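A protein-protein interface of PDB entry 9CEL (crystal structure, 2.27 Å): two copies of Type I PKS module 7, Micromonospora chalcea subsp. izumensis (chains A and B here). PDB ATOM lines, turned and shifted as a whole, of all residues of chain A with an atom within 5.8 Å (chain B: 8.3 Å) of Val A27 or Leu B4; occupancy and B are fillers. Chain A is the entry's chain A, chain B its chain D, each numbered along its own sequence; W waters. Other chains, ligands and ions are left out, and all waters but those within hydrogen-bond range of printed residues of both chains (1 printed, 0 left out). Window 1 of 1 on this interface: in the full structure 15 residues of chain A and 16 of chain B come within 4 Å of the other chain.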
ATOM      1  N   ALA A   3      15.142  -5.224   0.968  1.00  0.00           N
ATOM      2  CA  ALA A   3      14.745  -6.039   2.117  1.00  0.00           C
ATOM      3  C   ALA A   3      15.455  -7.378   2.122  1.00  0.00           C
ATOM      4  O   ALA A   3      15.762  -7.922   3.191  1.00  0.00           O
ATOM      5  CB  ALA A   3      13.237  -6.256   2.129  1.00  0.00           C
ATOM      6  N   LEU A   4      15.704  -7.928   0.938  1.00  0.00           N
ATOM      7  CA  LEU A   4      16.506  -9.132   0.831  1.00  0.00           C
ATOM      8  C   LEU A   4      17.952  -8.877   1.233  1.00  0.00           C
ATOM      9  O   LEU A   4      18.614  -9.777   1.753  1.00  0.00           O
ATOM     10  CB  LEU A   4      16.443  -9.660  -0.594  1.00  0.00           C
ATOM     11  CG  LEU A   4      15.146 -10.392  -0.899  1.00  0.00           C
ATOM     12  CD1 LEU A   4      15.209 -10.982  -2.281  1.00  0.00           C
ATOM     13  CD2 LEU A   4      14.883 -11.465   0.150  1.00  0.00           C
ATOM     14  N   GLU A  22      17.555 -20.466   2.599  1.00  0.00           N
ATOM     15  CA  GLU A  22      16.347 -21.192   2.222  1.00  0.00           C
ATOM     16  C   GLU A  22      15.277 -20.245   1.710  1.00  0.00           C
ATOM     17  O   GLU A  22      14.587 -20.548   0.732  1.00  0.00           O
ATOM     18  CB  GLU A  22      15.809 -22.005   3.406  1.00  0.00           C
ATOM     19  CG  GLU A  22      16.401 -23.389   3.508  1.00  0.00           C
ATOM     20  CD  GLU A  22      16.361 -24.116   2.182  1.00  0.00           C
ATOM     21  OE1 GLU A  22      15.290 -24.076   1.512  1.00  0.00           O
ATOM     22  OE2 GLU A  22      17.412 -24.700   1.806  1.00  0.00           O
ATOM     23  N   VAL A  23      15.123 -19.096   2.369  1.00  0.00           N
ATOM     24  CA  VAL A  23      14.156 -18.104   1.914  1.00  0.00           C
ATOM     25  C   VAL A  23      14.547 -17.570   0.542  1.00  0.00           C
ATOM     26  O   VAL A  23      13.689 -17.368  -0.331  1.00  0.00           O
ATOM     27  CB  VAL A  23      14.033 -16.971   2.948  1.00  0.00           C
ATOM     28  CG1 VAL A  23      13.431 -15.710   2.315  1.00  0.00           C
ATOM     29  CG2 VAL A  23      13.205 -17.431   4.115  1.00  0.00           C
ATOM     30  N   LEU A  24      15.847 -17.317   0.336  1.00  0.00           N
ATOM     31  CA  LEU A  24      16.311 -16.851  -0.964  1.00  0.00           C
ATOM     32  C   LEU A  24      16.007 -17.866  -2.054  1.00  0.00           C
ATOM     33  O   LEU A  24      15.729 -17.489  -3.196  1.00  0.00           O
ATOM     34  CB  LEU A  24      17.807 -16.563  -0.918  1.00  0.00           C
ATOM     35  CG  LEU A  24      18.135 -15.293  -0.138  1.00  0.00           C
ATOM     36  CD1 LEU A  24      19.603 -15.262   0.189  1.00  0.00           C
ATOM     37  CD2 LEU A  24      17.715 -14.033  -0.899  1.00  0.00           C
ATOM     38  N   GLY A  25      16.102 -19.157  -1.728  1.00  0.00           N
ATOM     39  CA  GLY A  25      15.822 -20.178  -2.718  1.00  0.00           C
ATOM     40  C   GLY A  25      14.366 -20.169  -3.154  1.00  0.00           C
ATOM     41  O   GLY A  25      14.060 -20.367  -4.329  1.00  0.00           O
ATOM     42  N   THR A  26      13.449 -19.939  -2.221  1.00  0.00           N
ATOM     43  CA  THR A  26      12.053 -19.880  -2.631  1.00  0.00           C
ATOM     44  C   THR A  26      11.778 -18.616  -3.430  1.00  0.00           C
ATOM     45  O   THR A  26      11.064 -18.661  -4.441  1.00  0.00           O
ATOM     46  CB  THR A  26      11.147 -19.985  -1.413  1.00  0.00           C
ATOM     47  OG1 THR A  26      11.528 -18.989  -0.462  1.00  0.00           O
ATOM     48  CG2 THR A  26      11.308 -21.357  -0.780  1.00  0.00           C
ATOM     49  N   VAL A  27      12.373 -17.484  -3.034  1.00  0.00           N
ATOM     50  CA  VAL A  27      12.232 -16.289  -3.863  1.00  0.00           C
ATOM     51  C   VAL A  27      12.727 -16.581  -5.266  1.00  0.00           C
ATOM     52  O   VAL A  27      12.111 -16.173  -6.257  1.00  0.00           O
ATOM     53  CB  VAL A  27      12.980 -15.082  -3.268  1.00  0.00           C
ATOM     54  CG1 VAL A  27      12.881 -13.920  -4.245  1.00  0.00           C
ATOM     55  CG2 VAL A  27      12.415 -14.672  -1.890  1.00  0.00           C
ATOM     56  N   ALA A  28      13.825 -17.338  -5.368  1.00  0.00           N
ATOM     57  CA  ALA A  28      14.434 -17.620  -6.657  1.00  0.00           C
ATOM     58  C   ALA A  28      13.539 -18.476  -7.553  1.00  0.00           C
ATOM     59  O   ALA A  28      13.660 -18.405  -8.777  1.00  0.00           O
ATOM     60  CB  ALA A  28      15.770 -18.311  -6.454  1.00  0.00           C
ATOM     61  N   THR A  29      12.647 -19.291  -6.975  1.00  0.00           N
ATOM     62  CA  THR A  29      11.687 -20.029  -7.792  1.00  0.00           C
ATOM     63  C   THR A  29      10.676 -19.121  -8.494  1.00  0.00           C
ATOM     64  O   THR A  29       9.782 -19.632  -9.183  1.00  0.00           O
ATOM     65  CB  THR A  29      10.916 -21.060  -6.957  1.00  0.00           C
ATOM     66  OG1 THR A  29       9.983 -20.391  -6.101  1.00  0.00           O
ATOM     67  CG2 THR A  29      11.864 -21.918  -6.122  1.00  0.00           C
ATOM     68  N   PHE A  30      10.764 -17.807  -8.334  1.00  0.00           N
ATOM     69  CA  PHE A  30       9.888 -16.898  -9.052  1.00  0.00           C
ATOM     70  C   PHE A  30      10.597 -16.207 -10.192  1.00  0.00           C
ATOM     71  O   PHE A  30       9.984 -15.393 -10.885  1.00  0.00           O
ATOM     72  CB  PHE A  30       9.308 -15.866  -8.092  1.00  0.00           C
ATOM     73  CG  PHE A  30       8.312 -16.442  -7.163  1.00  0.00           C
ATOM     74  CD1 PHE A  30       8.720 -17.033  -5.979  1.00  0.00           C
ATOM     75  CD2 PHE A  30       6.961 -16.433  -7.486  1.00  0.00           C
ATOM     76  CE1 PHE A  30       7.805 -17.591  -5.120  1.00  0.00           C
ATOM     77  CE2 PHE A  30       6.031 -16.993  -6.641  1.00  0.00           C
ATOM     78  CZ  PHE A  30       6.443 -17.576  -5.458  1.00  0.00           C
ATOM     79  N   ARG A  31      11.864 -16.526 -10.404  1.00  0.00           N
ATOM     80  CA  ARG A  31      12.742 -15.898 -11.360  1.00  0.00           C
ATOM     81  C   ARG A  31      12.614 -16.596 -12.701  1.00  0.00           C
ATOM     82  O   ARG A  31      12.467 -17.818 -12.743  1.00  0.00           O
ATOM     83  CB  ARG A  31      14.210 -15.967 -10.876  1.00  0.00           C
ATOM     84  CG  ARG A  31      14.655 -14.725 -10.102  1.00  0.00           C
ATOM     85  CD  ARG A  31      16.154 -14.753  -9.710  1.00  0.00           C
ATOM     86  NE  ARG A  31      17.005 -14.713 -10.893  1.00  0.00           N
ATOM     87  CZ  ARG A  31      18.314 -14.523 -10.870  1.00  0.00           C
ATOM     88  NH1 ARG A  31      18.976 -14.394  -9.724  1.00  0.00           N
ATOM     89  NH2 ARG A  31      18.975 -14.461 -12.022  1.00  0.00           N
ATOM     90  N   ASP A 188      19.999  -8.256  -5.069  1.00  0.00           N
ATOM     91  CA  ASP A 188      18.993  -9.317  -5.009  1.00  0.00           C
ATOM     92  C   ASP A 188      19.277 -10.439  -6.013  1.00  0.00           C
ATOM     93  O   ASP A 188      19.033 -11.616  -5.717  1.00  0.00           O
ATOM     94  CB  ASP A 188      17.598  -8.728  -5.246  1.00  0.00           C
ATOM     95  CG  ASP A 188      17.069  -7.932  -4.050  1.00  0.00           C
ATOM     96  OD1 ASP A 188      17.817  -7.716  -3.077  1.00  0.00           O
ATOM     97  OD2 ASP A 188      15.892  -7.515  -4.090  1.00  0.00           O
ATOM     98  N   THR A 192      19.506 -14.076  -4.723  1.00  0.00           N
ATOM     99  CA  THR A 192      18.602 -15.139  -5.155  1.00  0.00           C
ATOM    100  C   THR A 192      19.359 -16.185  -5.945  1.00  0.00           C
ATOM    101  O   THR A 192      19.041 -17.377  -5.843  1.00  0.00           O
ATOM    102  CB  THR A 192      17.431 -14.592  -5.969  1.00  0.00           C
ATOM    103  OG1 THR A 192      17.922 -13.648  -6.925  1.00  0.00           O
ATOM    104  CG2 THR A 192      16.481 -13.896  -5.059  1.00  0.00           C
ATOM    105  N   GLY B   1      12.368  -3.723 -10.998  1.00  0.00           N
ATOM    106  CA  GLY B   1      12.016  -3.930  -9.602  1.00  0.00           C
ATOM    107  C   GLY B   1      12.971  -4.826  -8.825  1.00  0.00           C
ATOM    108  O   GLY B   1      13.820  -5.496  -9.421  1.00  0.00           O
ATOM    109  N   SER B   2      12.846  -4.821  -7.494  1.00  0.00           N
ATOM    110  CA  SER B   2      13.604  -5.716  -6.622  1.00  0.00           C
ATOM    111  C   SER B   2      13.100  -7.153  -6.764  1.00  0.00           C
ATOM    112  O   SER B   2      12.029  -7.405  -7.311  1.00  0.00           O
ATOM    113  CB  SER B   2      13.473  -5.281  -5.163  1.00  0.00           C
ATOM    114  OG  SER B   2      12.324  -5.868  -4.557  1.00  0.00           O
ATOM    115  N   ALA B   3      13.869  -8.112  -6.230  1.00  0.00           N
ATOM    116  CA  ALA B   3      13.463  -9.511  -6.380  1.00  0.00           C
ATOM    117  C   ALA B   3      12.178  -9.836  -5.632  1.00  0.00           C
ATOM    118  O   ALA B   3      11.510 -10.826  -5.957  1.00  0.00           O
ATOM    119  CB  ALA B   3      14.563 -10.464  -5.908  1.00  0.00           C
ATOM    120  N   LEU B   4      11.826  -9.060  -4.618  1.00  0.00           N
ATOM    121  CA  LEU B   4      10.564  -9.315  -3.947  1.00  0.00           C
ATOM    122  C   LEU B   4       9.406  -8.779  -4.768  1.00  0.00           C
ATOM    123  O   LEU B   4       8.322  -9.368  -4.773  1.00  0.00           O
ATOM    124  CB  LEU B   4      10.581  -8.683  -2.560  1.00  0.00           C
ATOM    125  CG  LEU B   4      11.584  -9.377  -1.642  1.00  0.00           C
ATOM    126  CD1 LEU B   4      11.541  -8.791  -0.248  1.00  0.00           C
ATOM    127  CD2 LEU B   4      11.299 -10.866  -1.603  1.00  0.00           C
ATOM    128  N   VAL B   5       9.636  -7.652  -5.438  1.00  0.00           N
ATOM    129  CA  VAL B   5       8.638  -7.047  -6.302  1.00  0.00           C
ATOM    130  C   VAL B   5       8.326  -7.980  -7.457  1.00  0.00           C
ATOM    131  O   VAL B   5       7.173  -8.339  -7.682  1.00  0.00           O
ATOM    132  CB  VAL B   5       9.140  -5.680  -6.794  1.00  0.00           C
ATOM    133  CG1 VAL B   5       8.242  -5.133  -7.897  1.00  0.00           C
ATOM    134  CG2 VAL B   5       9.246  -4.718  -5.615  1.00  0.00           C
ATOM    135  N   GLU B   6       9.357  -8.435  -8.166  1.00  0.00           N
ATOM    136  CA  GLU B   6       9.128  -9.407  -9.225  1.00  0.00           C
ATOM    137  C   GLU B   6       8.552 -10.699  -8.674  1.00  0.00           C
ATOM    138  O   GLU B   6       7.740 -11.352  -9.336  1.00  0.00           O
ATOM    139  CB  GLU B   6      10.431  -9.675  -9.986  1.00  0.00           C
ATOM    140  CG  GLU B   6      11.093  -8.401 -10.497  1.00  0.00           C
ATOM    141  CD  GLU B   6      10.189  -7.579 -11.418  1.00  0.00           C
ATOM    142  OE1 GLU B   6       9.228  -8.140 -11.989  1.00  0.00           O
ATOM    143  OE2 GLU B   6      10.439  -6.364 -11.575  1.00  0.00           O
ATOM    144  N   MET B   7       8.951 -11.094  -7.472  1.00  0.00           N
ATOM    145  CA  MET B   7       8.331 -12.273  -6.901  1.00  0.00           C
ATOM    146  C   MET B   7       6.831 -12.084  -6.829  1.00  0.00           C
ATOM    147  O   MET B   7       6.062 -12.895  -7.362  1.00  0.00           O
ATOM    148  CB  MET B   7       8.882 -12.579  -5.517  1.00  0.00           C
ATOM    149  CG  MET B   7       8.235 -13.824  -4.951  1.00  0.00           C
ATOM    150  SD  MET B   7       8.560 -14.116  -3.205  1.00  0.00           S
ATOM    151  CE  MET B   7       7.888 -12.636  -2.464  1.00  0.00           C
ATOM    152  N   TYR B   8       6.401 -10.973  -6.230  1.00  0.00           N
ATOM    153  CA  TYR B   8       4.989 -10.836  -5.912  1.00  0.00           C
ATOM    154  C   TYR B   8       4.132 -10.729  -7.169  1.00  0.00           C
ATOM    155  O   TYR B   8       3.001 -11.219  -7.185  1.00  0.00           O
ATOM    156  CB  TYR B   8       4.765  -9.633  -5.015  1.00  0.00           C
ATOM    157  CG  TYR B   8       3.318  -9.445  -4.640  1.00  0.00           C
ATOM    158  CD1 TYR B   8       2.692 -10.298  -3.730  1.00  0.00           C
ATOM    159  CD2 TYR B   8       2.575  -8.409  -5.186  1.00  0.00           C
ATOM    160  CE1 TYR B   8       1.355 -10.123  -3.388  1.00  0.00           C
ATOM    161  CE2 TYR B   8       1.233  -8.225  -4.838  1.00  0.00           C
ATOM    162  CZ  TYR B   8       0.636  -9.083  -3.950  1.00  0.00           C
ATOM    163  OH  TYR B   8      -0.689  -8.895  -3.620  1.00  0.00           O
ATOM    164  N   ARG B   9       4.645 -10.101  -8.225  1.00  0.00           N
ATOM    165  CA  ARG B   9       3.847  -9.984  -9.437  1.00  0.00           C
ATOM    166  C   ARG B   9       3.845 -11.288 -10.229  1.00  0.00           C
ATOM    167  O   ARG B   9       2.781 -11.741 -10.659  1.00  0.00           O
ATOM    168  CB  ARG B   9       4.319  -8.793 -10.276  1.00  0.00           C
ATOM    169  CG  ARG B   9       5.355  -9.079 -11.338  1.00  0.00           C
ATOM    170  CD  ARG B   9       5.418  -7.945 -12.341  1.00  0.00           C
ATOM    171  NE  ARG B   9       6.277  -6.845 -11.907  1.00  0.00           N
ATOM    172  CZ  ARG B   9       5.880  -5.789 -11.203  1.00  0.00           C
ATOM    173  NH1 ARG B   9       4.632  -5.669 -10.764  1.00  0.00           N
ATOM    174  NH2 ARG B   9       6.756  -4.820 -10.939  1.00  0.00           N
ATOM    175  N   ARG B  10       4.999 -11.936 -10.400  1.00  0.00           N
ATOM    176  CA  ARG B  10       4.985 -13.278 -10.963  1.00  0.00           C
ATOM    177  C   ARG B  10       4.104 -14.208 -10.135  1.00  0.00           C
ATOM    178  O   ARG B  10       3.536 -15.170 -10.668  1.00  0.00           O
ATOM    179  CB  ARG B  10       6.419 -13.830 -11.073  1.00  0.00           C
ATOM    180  CG  ARG B  10       6.513 -15.272 -11.588  1.00  0.00           C
ATOM    181  CD  ARG B  10       7.260 -15.386 -12.948  1.00  0.00           C
ATOM    182  NE  ARG B  10       7.900 -16.693 -13.111  1.00  0.00           N
ATOM    183  CZ  ARG B  10       8.965 -16.927 -13.870  1.00  0.00           C
ATOM    184  NH1 ARG B  10       9.511 -15.978 -14.615  1.00  0.00           N
ATOM    185  NH2 ARG B  10       9.504 -18.146 -13.880  1.00  0.00           N
ATOM    186  N   ALA B  11       3.947 -13.923  -8.846  1.00  0.00           N
ATOM    187  CA  ALA B  11       3.193 -14.821  -7.981  1.00  0.00           C
ATOM    188  C   ALA B  11       1.697 -14.701  -8.224  1.00  0.00           C
ATOM    189  O   ALA B  11       0.972 -15.703  -8.199  1.00  0.00           O
ATOM    190  CB  ALA B  11       3.508 -14.529  -6.516  1.00  0.00           C
ATOM    191  N   ARG B  16       0.290 -18.038  -7.272  1.00  0.00           N
ATOM    192  CA  ARG B  16       1.203 -18.412  -6.209  1.00  0.00           C
ATOM    193  C   ARG B  16       1.261 -17.343  -5.126  1.00  0.00           C
ATOM    194  O   ARG B  16       2.219 -17.291  -4.343  1.00  0.00           O
ATOM    195  CB  ARG B  16       2.582 -18.683  -6.799  1.00  0.00           C
ATOM    196  CG  ARG B  16       2.633 -19.898  -7.721  1.00  0.00           C
ATOM    197  CD  ARG B  16       4.069 -20.123  -8.244  1.00  0.00           C
ATOM    198  NE  ARG B  16       4.996 -20.510  -7.182  1.00  0.00           N
ATOM    199  CZ  ARG B  16       6.323 -20.453  -7.272  1.00  0.00           C
ATOM    200  NH1 ARG B  16       6.927 -20.008  -8.363  1.00  0.00           N
ATOM    201  NH2 ARG B  16       7.062 -20.836  -6.230  1.00  0.00           N
ATOM    202  N   GLU B  19       1.805 -18.453  -1.489  1.00  0.00           N
ATOM    203  CA  GLU B  19       3.179 -18.819  -1.175  1.00  0.00           C
ATOM    204  C   GLU B  19       4.043 -17.576  -1.009  1.00  0.00           C
ATOM    205  O   GLU B  19       4.873 -17.506  -0.094  1.00  0.00           O
ATOM    206  CB  GLU B  19       3.758 -19.739  -2.249  1.00  0.00           C
ATOM    207  CG  GLU B  19       5.071 -20.372  -1.819  1.00  0.00           C
ATOM    208  CD  GLU B  19       5.659 -21.336  -2.835  1.00  0.00           C
ATOM    209  OE1 GLU B  19       5.099 -21.465  -3.952  1.00  0.00           O
ATOM    210  OE2 GLU B  19       6.692 -21.966  -2.501  1.00  0.00           O
ATOM    211  N   ALA B  20       3.835 -16.568  -1.864  1.00  0.00           N
ATOM    212  CA  ALA B  20       4.631 -15.350  -1.769  1.00  0.00           C
ATOM    213  C   ALA B  20       4.364 -14.604  -0.463  1.00  0.00           C
ATOM    214  O   ALA B  20       5.290 -14.053   0.141  1.00  0.00           O
ATOM    215  CB  ALA B  20       4.359 -14.448  -2.969  1.00  0.00           C
ATOM    216  N   VAL B  23       6.498 -16.385   2.250  1.00  0.00           N
ATOM    217  CA  VAL B  23       7.881 -15.954   2.053  1.00  0.00           C
ATOM    218  C   VAL B  23       8.095 -14.571   2.649  1.00  0.00           C
ATOM    219  O   VAL B  23       9.070 -14.322   3.374  1.00  0.00           O
ATOM    220  CB  VAL B  23       8.229 -15.962   0.550  1.00  0.00           C
ATOM    221  CG1 VAL B  23       9.334 -14.980   0.259  1.00  0.00           C
ATOM    222  CG2 VAL B  23       8.604 -17.341   0.086  1.00  0.00           C
ATOM    223  N   LEU B  24       7.180 -13.652   2.346  1.00  0.00           N
ATOM    224  CA  LEU B  24       7.362 -12.262   2.741  1.00  0.00           C
ATOM    225  C   LEU B  24       7.292 -12.104   4.248  1.00  0.00           C
ATOM    226  O   LEU B  24       8.065 -11.326   4.831  1.00  0.00           O
ATOM    227  CB  LEU B  24       6.325 -11.369   2.067  1.00  0.00           C
ATOM    228  CG  LEU B  24       6.663 -11.028   0.619  1.00  0.00           C
ATOM    229  CD1 LEU B  24       5.453 -10.458  -0.091  1.00  0.00           C
ATOM    230  CD2 LEU B  24       7.839 -10.053   0.596  1.00  0.00           C
ATOM    231  N   VAL B  27      10.750 -13.058   5.561  1.00  0.00           N
ATOM    232  CA  VAL B  27      11.673 -11.935   5.387  1.00  0.00           C
ATOM    233  C   VAL B  27      11.356 -10.810   6.370  1.00  0.00           C
ATOM    234  O   VAL B  27      12.263 -10.147   6.889  1.00  0.00           O
ATOM    235  CB  VAL B  27      11.620 -11.451   3.928  1.00  0.00           C
ATOM    236  CG1 VAL B  27      12.302 -10.107   3.758  1.00  0.00           C
ATOM    237  CG2 VAL B  27      12.216 -12.492   3.024  1.00  0.00           C
ATOM    238  N   ALA B  28      10.068 -10.569   6.641  1.00  0.00           N
ATOM    239  CA  ALA B  28       9.691  -9.479   7.533  1.00  0.00           C
ATOM    240  C   ALA B  28      10.282  -9.641   8.932  1.00  0.00           C
ATOM    241  O   ALA B  28      10.501  -8.642   9.622  1.00  0.00           O
ATOM    242  CB  ALA B  28       8.163  -9.364   7.635  1.00  0.00           C
ATOM    243  N   ARG B  31      13.443  -7.504   9.890  1.00  0.00           N
ATOM    244  CA  ARG B  31      13.223  -6.066   9.883  1.00  0.00           C
ATOM    245  C   ARG B  31      13.133  -5.546  11.315  1.00  0.00           C
ATOM    246  O   ARG B  31      12.663  -6.260  12.204  1.00  0.00           O
ATOM    247  CB  ARG B  31      11.910  -5.719   9.135  1.00  0.00           C
ATOM    248  CG  ARG B  31      11.989  -5.670   7.592  1.00  0.00           C
ATOM    249  CD  ARG B  31      10.650  -5.222   6.972  1.00  0.00           C
ATOM    250  NE  ARG B  31      10.135  -4.056   7.673  1.00  0.00           N
ATOM    251  CZ  ARG B  31       9.102  -3.317   7.290  1.00  0.00           C
ATOM    252  NH1 ARG B  31       8.376  -3.626   6.208  1.00  0.00           N
ATOM    253  NH2 ARG B  31       8.791  -2.236   8.006  1.00  0.00           N
ATOM    254  N   VAL B 186       4.199  -0.803  -5.567  1.00  0.00           N
ATOM    255  CA  VAL B 186       4.524  -1.526  -4.347  1.00  0.00           C
ATOM    256  C   VAL B 186       6.037  -1.575  -4.186  1.00  0.00           C
ATOM    257  O   VAL B 186       6.805  -1.344  -5.125  1.00  0.00           O
ATOM    258  CB  VAL B 186       3.933  -2.946  -4.319  1.00  0.00           C
ATOM    259  CG1 VAL B 186       2.422  -2.881  -4.182  1.00  0.00           C
ATOM    260  CG2 VAL B 186       4.331  -3.697  -5.568  1.00  0.00           C
ATOM    261  N   ASP B 187       6.458  -1.871  -2.962  1.00  0.00           N
ATOM    262  CA  ASP B 187       7.875  -1.938  -2.656  1.00  0.00           C
ATOM    263  C   ASP B 187       8.098  -2.976  -1.568  1.00  0.00           C
ATOM    264  O   ASP B 187       7.155  -3.556  -1.018  1.00  0.00           O
ATOM    265  CB  ASP B 187       8.418  -0.560  -2.264  1.00  0.00           C
ATOM    266  CG  ASP B 187       7.671   0.067  -1.098  1.00  0.00           C
ATOM    267  OD1 ASP B 187       7.076  -0.658  -0.270  1.00  0.00           O
ATOM    268  OD2 ASP B 187       7.665   1.310  -1.006  1.00  0.00           O
ATOM    269  N   ASP B 188       9.378  -3.192  -1.260  1.00  0.00           N
ATOM    270  CA  ASP B 188       9.761  -4.130  -0.220  1.00  0.00           C
ATOM    271  C   ASP B 188       9.092  -3.822   1.110  1.00  0.00           C
ATOM    272  O   ASP B 188       8.626  -4.735   1.803  1.00  0.00           O
ATOM    273  CB  ASP B 188      11.282  -4.125  -0.066  1.00  0.00           C
ATOM    274  CG  ASP B 188      11.976  -4.799  -1.227  1.00  0.00           C
ATOM    275  OD1 ASP B 188      11.271  -5.220  -2.160  1.00  0.00           O
ATOM    276  OD2 ASP B 188      13.219  -4.915  -1.212  1.00  0.00           O
ATOM    277  N   THR B 189       9.061  -2.558   1.513  1.00  0.00           N
ATOM    278  CA  THR B 189       8.475  -2.258   2.819  1.00  0.00           C
ATOM    279  C   THR B 189       7.010  -2.679   2.860  1.00  0.00           C
ATOM    280  O   THR B 189       6.591  -3.425   3.756  1.00  0.00           O
ATOM    281  CB  THR B 189       8.615  -0.772   3.143  1.00  0.00           C
ATOM    282  OG1 THR B 189       9.903  -0.323   2.744  1.00  0.00           O
ATOM    283  CG2 THR B 189       8.412  -0.502   4.650  1.00  0.00           C
ATOM    284  N   LEU B 191       5.435  -4.773   0.800  1.00  0.00           N
ATOM    285  CA  LEU B 191       5.319  -6.214   0.649  1.00  0.00           C
ATOM    286  C   LEU B 191       5.663  -6.920   1.946  1.00  0.00           C
ATOM    287  O   LEU B 191       4.906  -7.783   2.405  1.00  0.00           O
ATOM    288  CB  LEU B 191       6.197  -6.705  -0.503  1.00  0.00           C
ATOM    289  CG  LEU B 191       5.673  -6.251  -1.875  1.00  0.00           C
ATOM    290  CD1 LEU B 191       6.758  -6.212  -2.918  1.00  0.00           C
ATOM    291  CD2 LEU B 191       4.488  -7.107  -2.372  1.00  0.00           C
ATOM    292  N   THR B 192       6.795  -6.551   2.573  1.00  0.00           N
ATOM    293  CA  THR B 192       7.179  -7.278   3.769  1.00  0.00           C
ATOM    294  C   THR B 192       6.196  -7.001   4.871  1.00  0.00           C
ATOM    295  O   THR B 192       5.884  -7.912   5.643  1.00  0.00           O
ATOM    296  CB  THR B 192       8.607  -6.946   4.215  1.00  0.00           C
ATOM    297  OG1 THR B 192       8.732  -5.545   4.491  1.00  0.00           O
ATOM    298  CG2 THR B 192       9.574  -7.357   3.126  1.00  0.00           C
HETATM  299  O   HOH W   1      14.420  -7.012  -1.999  1.00  0.00           O
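Ala A3 touches Asp B188, and with the chains exchanged Asp A188 touches Ala B3. Val A23 touches Val B27, and with the chains exchanged Val A27 touches Val B23. Val A27 touches Ala B3, but with the chains exchanged Ala A3 does not touch Val B27 (4.1 Å). Val A27 touches Leu B4, but with the chains exchanged Leu A4 does not touch Val B27 (4.1 Å). Of the 18 pairs that touch across the chains among the printed residues, 7 have their exchanged pair printed and touching as well.
Printed residues of chain B within 4 Å of Val A23: Val B27. Val A27 touches three residues of chain B. No residue of chain B comes within 4 Å of Ala A28. Of the printed residues of chain B, Arg A31 touches Arg B10 (3.2 Å). Leu B4 touches just these residues of chain A: Ala A3 (3.9 Å), Leu A4 (3.8 Å) and Val A27 (3.98 Å). Printed residues of chain A within 4 Å of Ala B11: Phe A30 (3.5 Å). Printed residues of chain A within 4 Å of Asp B188: Ala A3.
Leu B4 touches Ala A3 (CD1 to CB, 3.9 Å). CB of Ala A3 touches CG2 of Thr B192, at 3.95 Å. Leu A4 touches Ala B3. Leu A4 touches Leu B4. Val B23 touches Thr A26 (CG2 to OG1, 3.4 Å). CG1 of Val A27 touches O of Ala B3, 3.8 Å away. Val A27 touches Leu B4 (CG2 to CD2, 3.98 Å). Val A27 touches Val B23 (CG2 to CG1, 3.8 Å). Met B7 touches Phe A30 (CG to CD1, 3.4 Å). CB of Ala B11 touches CE2 of Phe A30 (3.5 Å).
Of the 25 printed residues of chain B, 11 touch a printed residue of chain A. Printed residues of chain B that touch a printed residue of chain A: Ser B2, Ala B3, Leu B4, Met B7, Arg B10, Ala B11, Arg B16, Val B23, Val B27, Asp B188 and Thr B192. Hydrophobic or aromatic side chains of chain B that line the printed part of chain A: Ala B3, Leu B4, Met B7, Ala B11, Val B23 and Val B27. Printed residues of chain A that touch a printed residue of chain B: Ala A3, Leu A4, Val A23, Thr A26, Val A27, Thr A29, Phe A30, Arg A31 and Asp A188. Hydrophobic or aromatic side chains of chain A within 4 Å of the printed part of chain B: Ala A3, Leu A4, Val A23, Val A27 and Phe A30. Among the printed residues, 18 pairs touch across the chains. Among the printed residues, no Asp or Glu carboxylate lies within 4 Å of a Lys or Arg side-chain nitrogen of the other chain.
Water W1 lies within hydrogen-bond range of the side-chain carboxylate (OD2) of Asp B188, the side-chain carboxylate (OD2) of Asp A188, the backbone NH (N) of Leu A4 and the side-chain hydroxyl (OG) of Ser B2.
The backbone carbonyl oxygen (O) of Arg A31 is in hydrogen-bond range of the guanidinium group (NH2) of Arg B10 (3.2 Å). The backbone carbonyl oxygen (O) of Phe A30 sits at hydrogen-bond distance from the guanidinium group (NE) of Arg B10, at 3.3 Å. N of Ala A3 lies within hydrogen-bond range of OD2 of Asp B188, at 2.9 Å. N of Ala B3 sits at hydrogen-bond distance from OD2 of Asp A188, at 3.0 Å. The side-chain hydroxyl (OG1) of Thr A29 sits at hydrogen-bond distance from the guanidinium group (NH2) of Arg B16 (3.0 Å).
NH1 of Arg A31 sits at hydrogen-bond distance from OG1 of Thr A192 (3.1 Å). The backbone carbonyl oxygen (O) of Thr A26 is in hydrogen-bond range of the side-chain hydroxyl (OG1) of Thr A29. The backbone carbonyl oxygen (O) of Thr B189 lies within hydrogen-bond range of the side-chain hydroxyl (OG1) of Thr B192 (3.1 Å). OG1 of Thr A26 is in hydrogen-bond range of O of Val A23, at 2.7 Å. The side-chain hydroxyl of Ser B2 sits at hydrogen-bond distance from the backbone NH of Val B5, 3.3 Å away. The side-chain hydroxyl (OG) of Ser B2 sits at hydrogen-bond distance from the side-chain carboxylate (OD1) of Asp B188 (2.7 Å).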
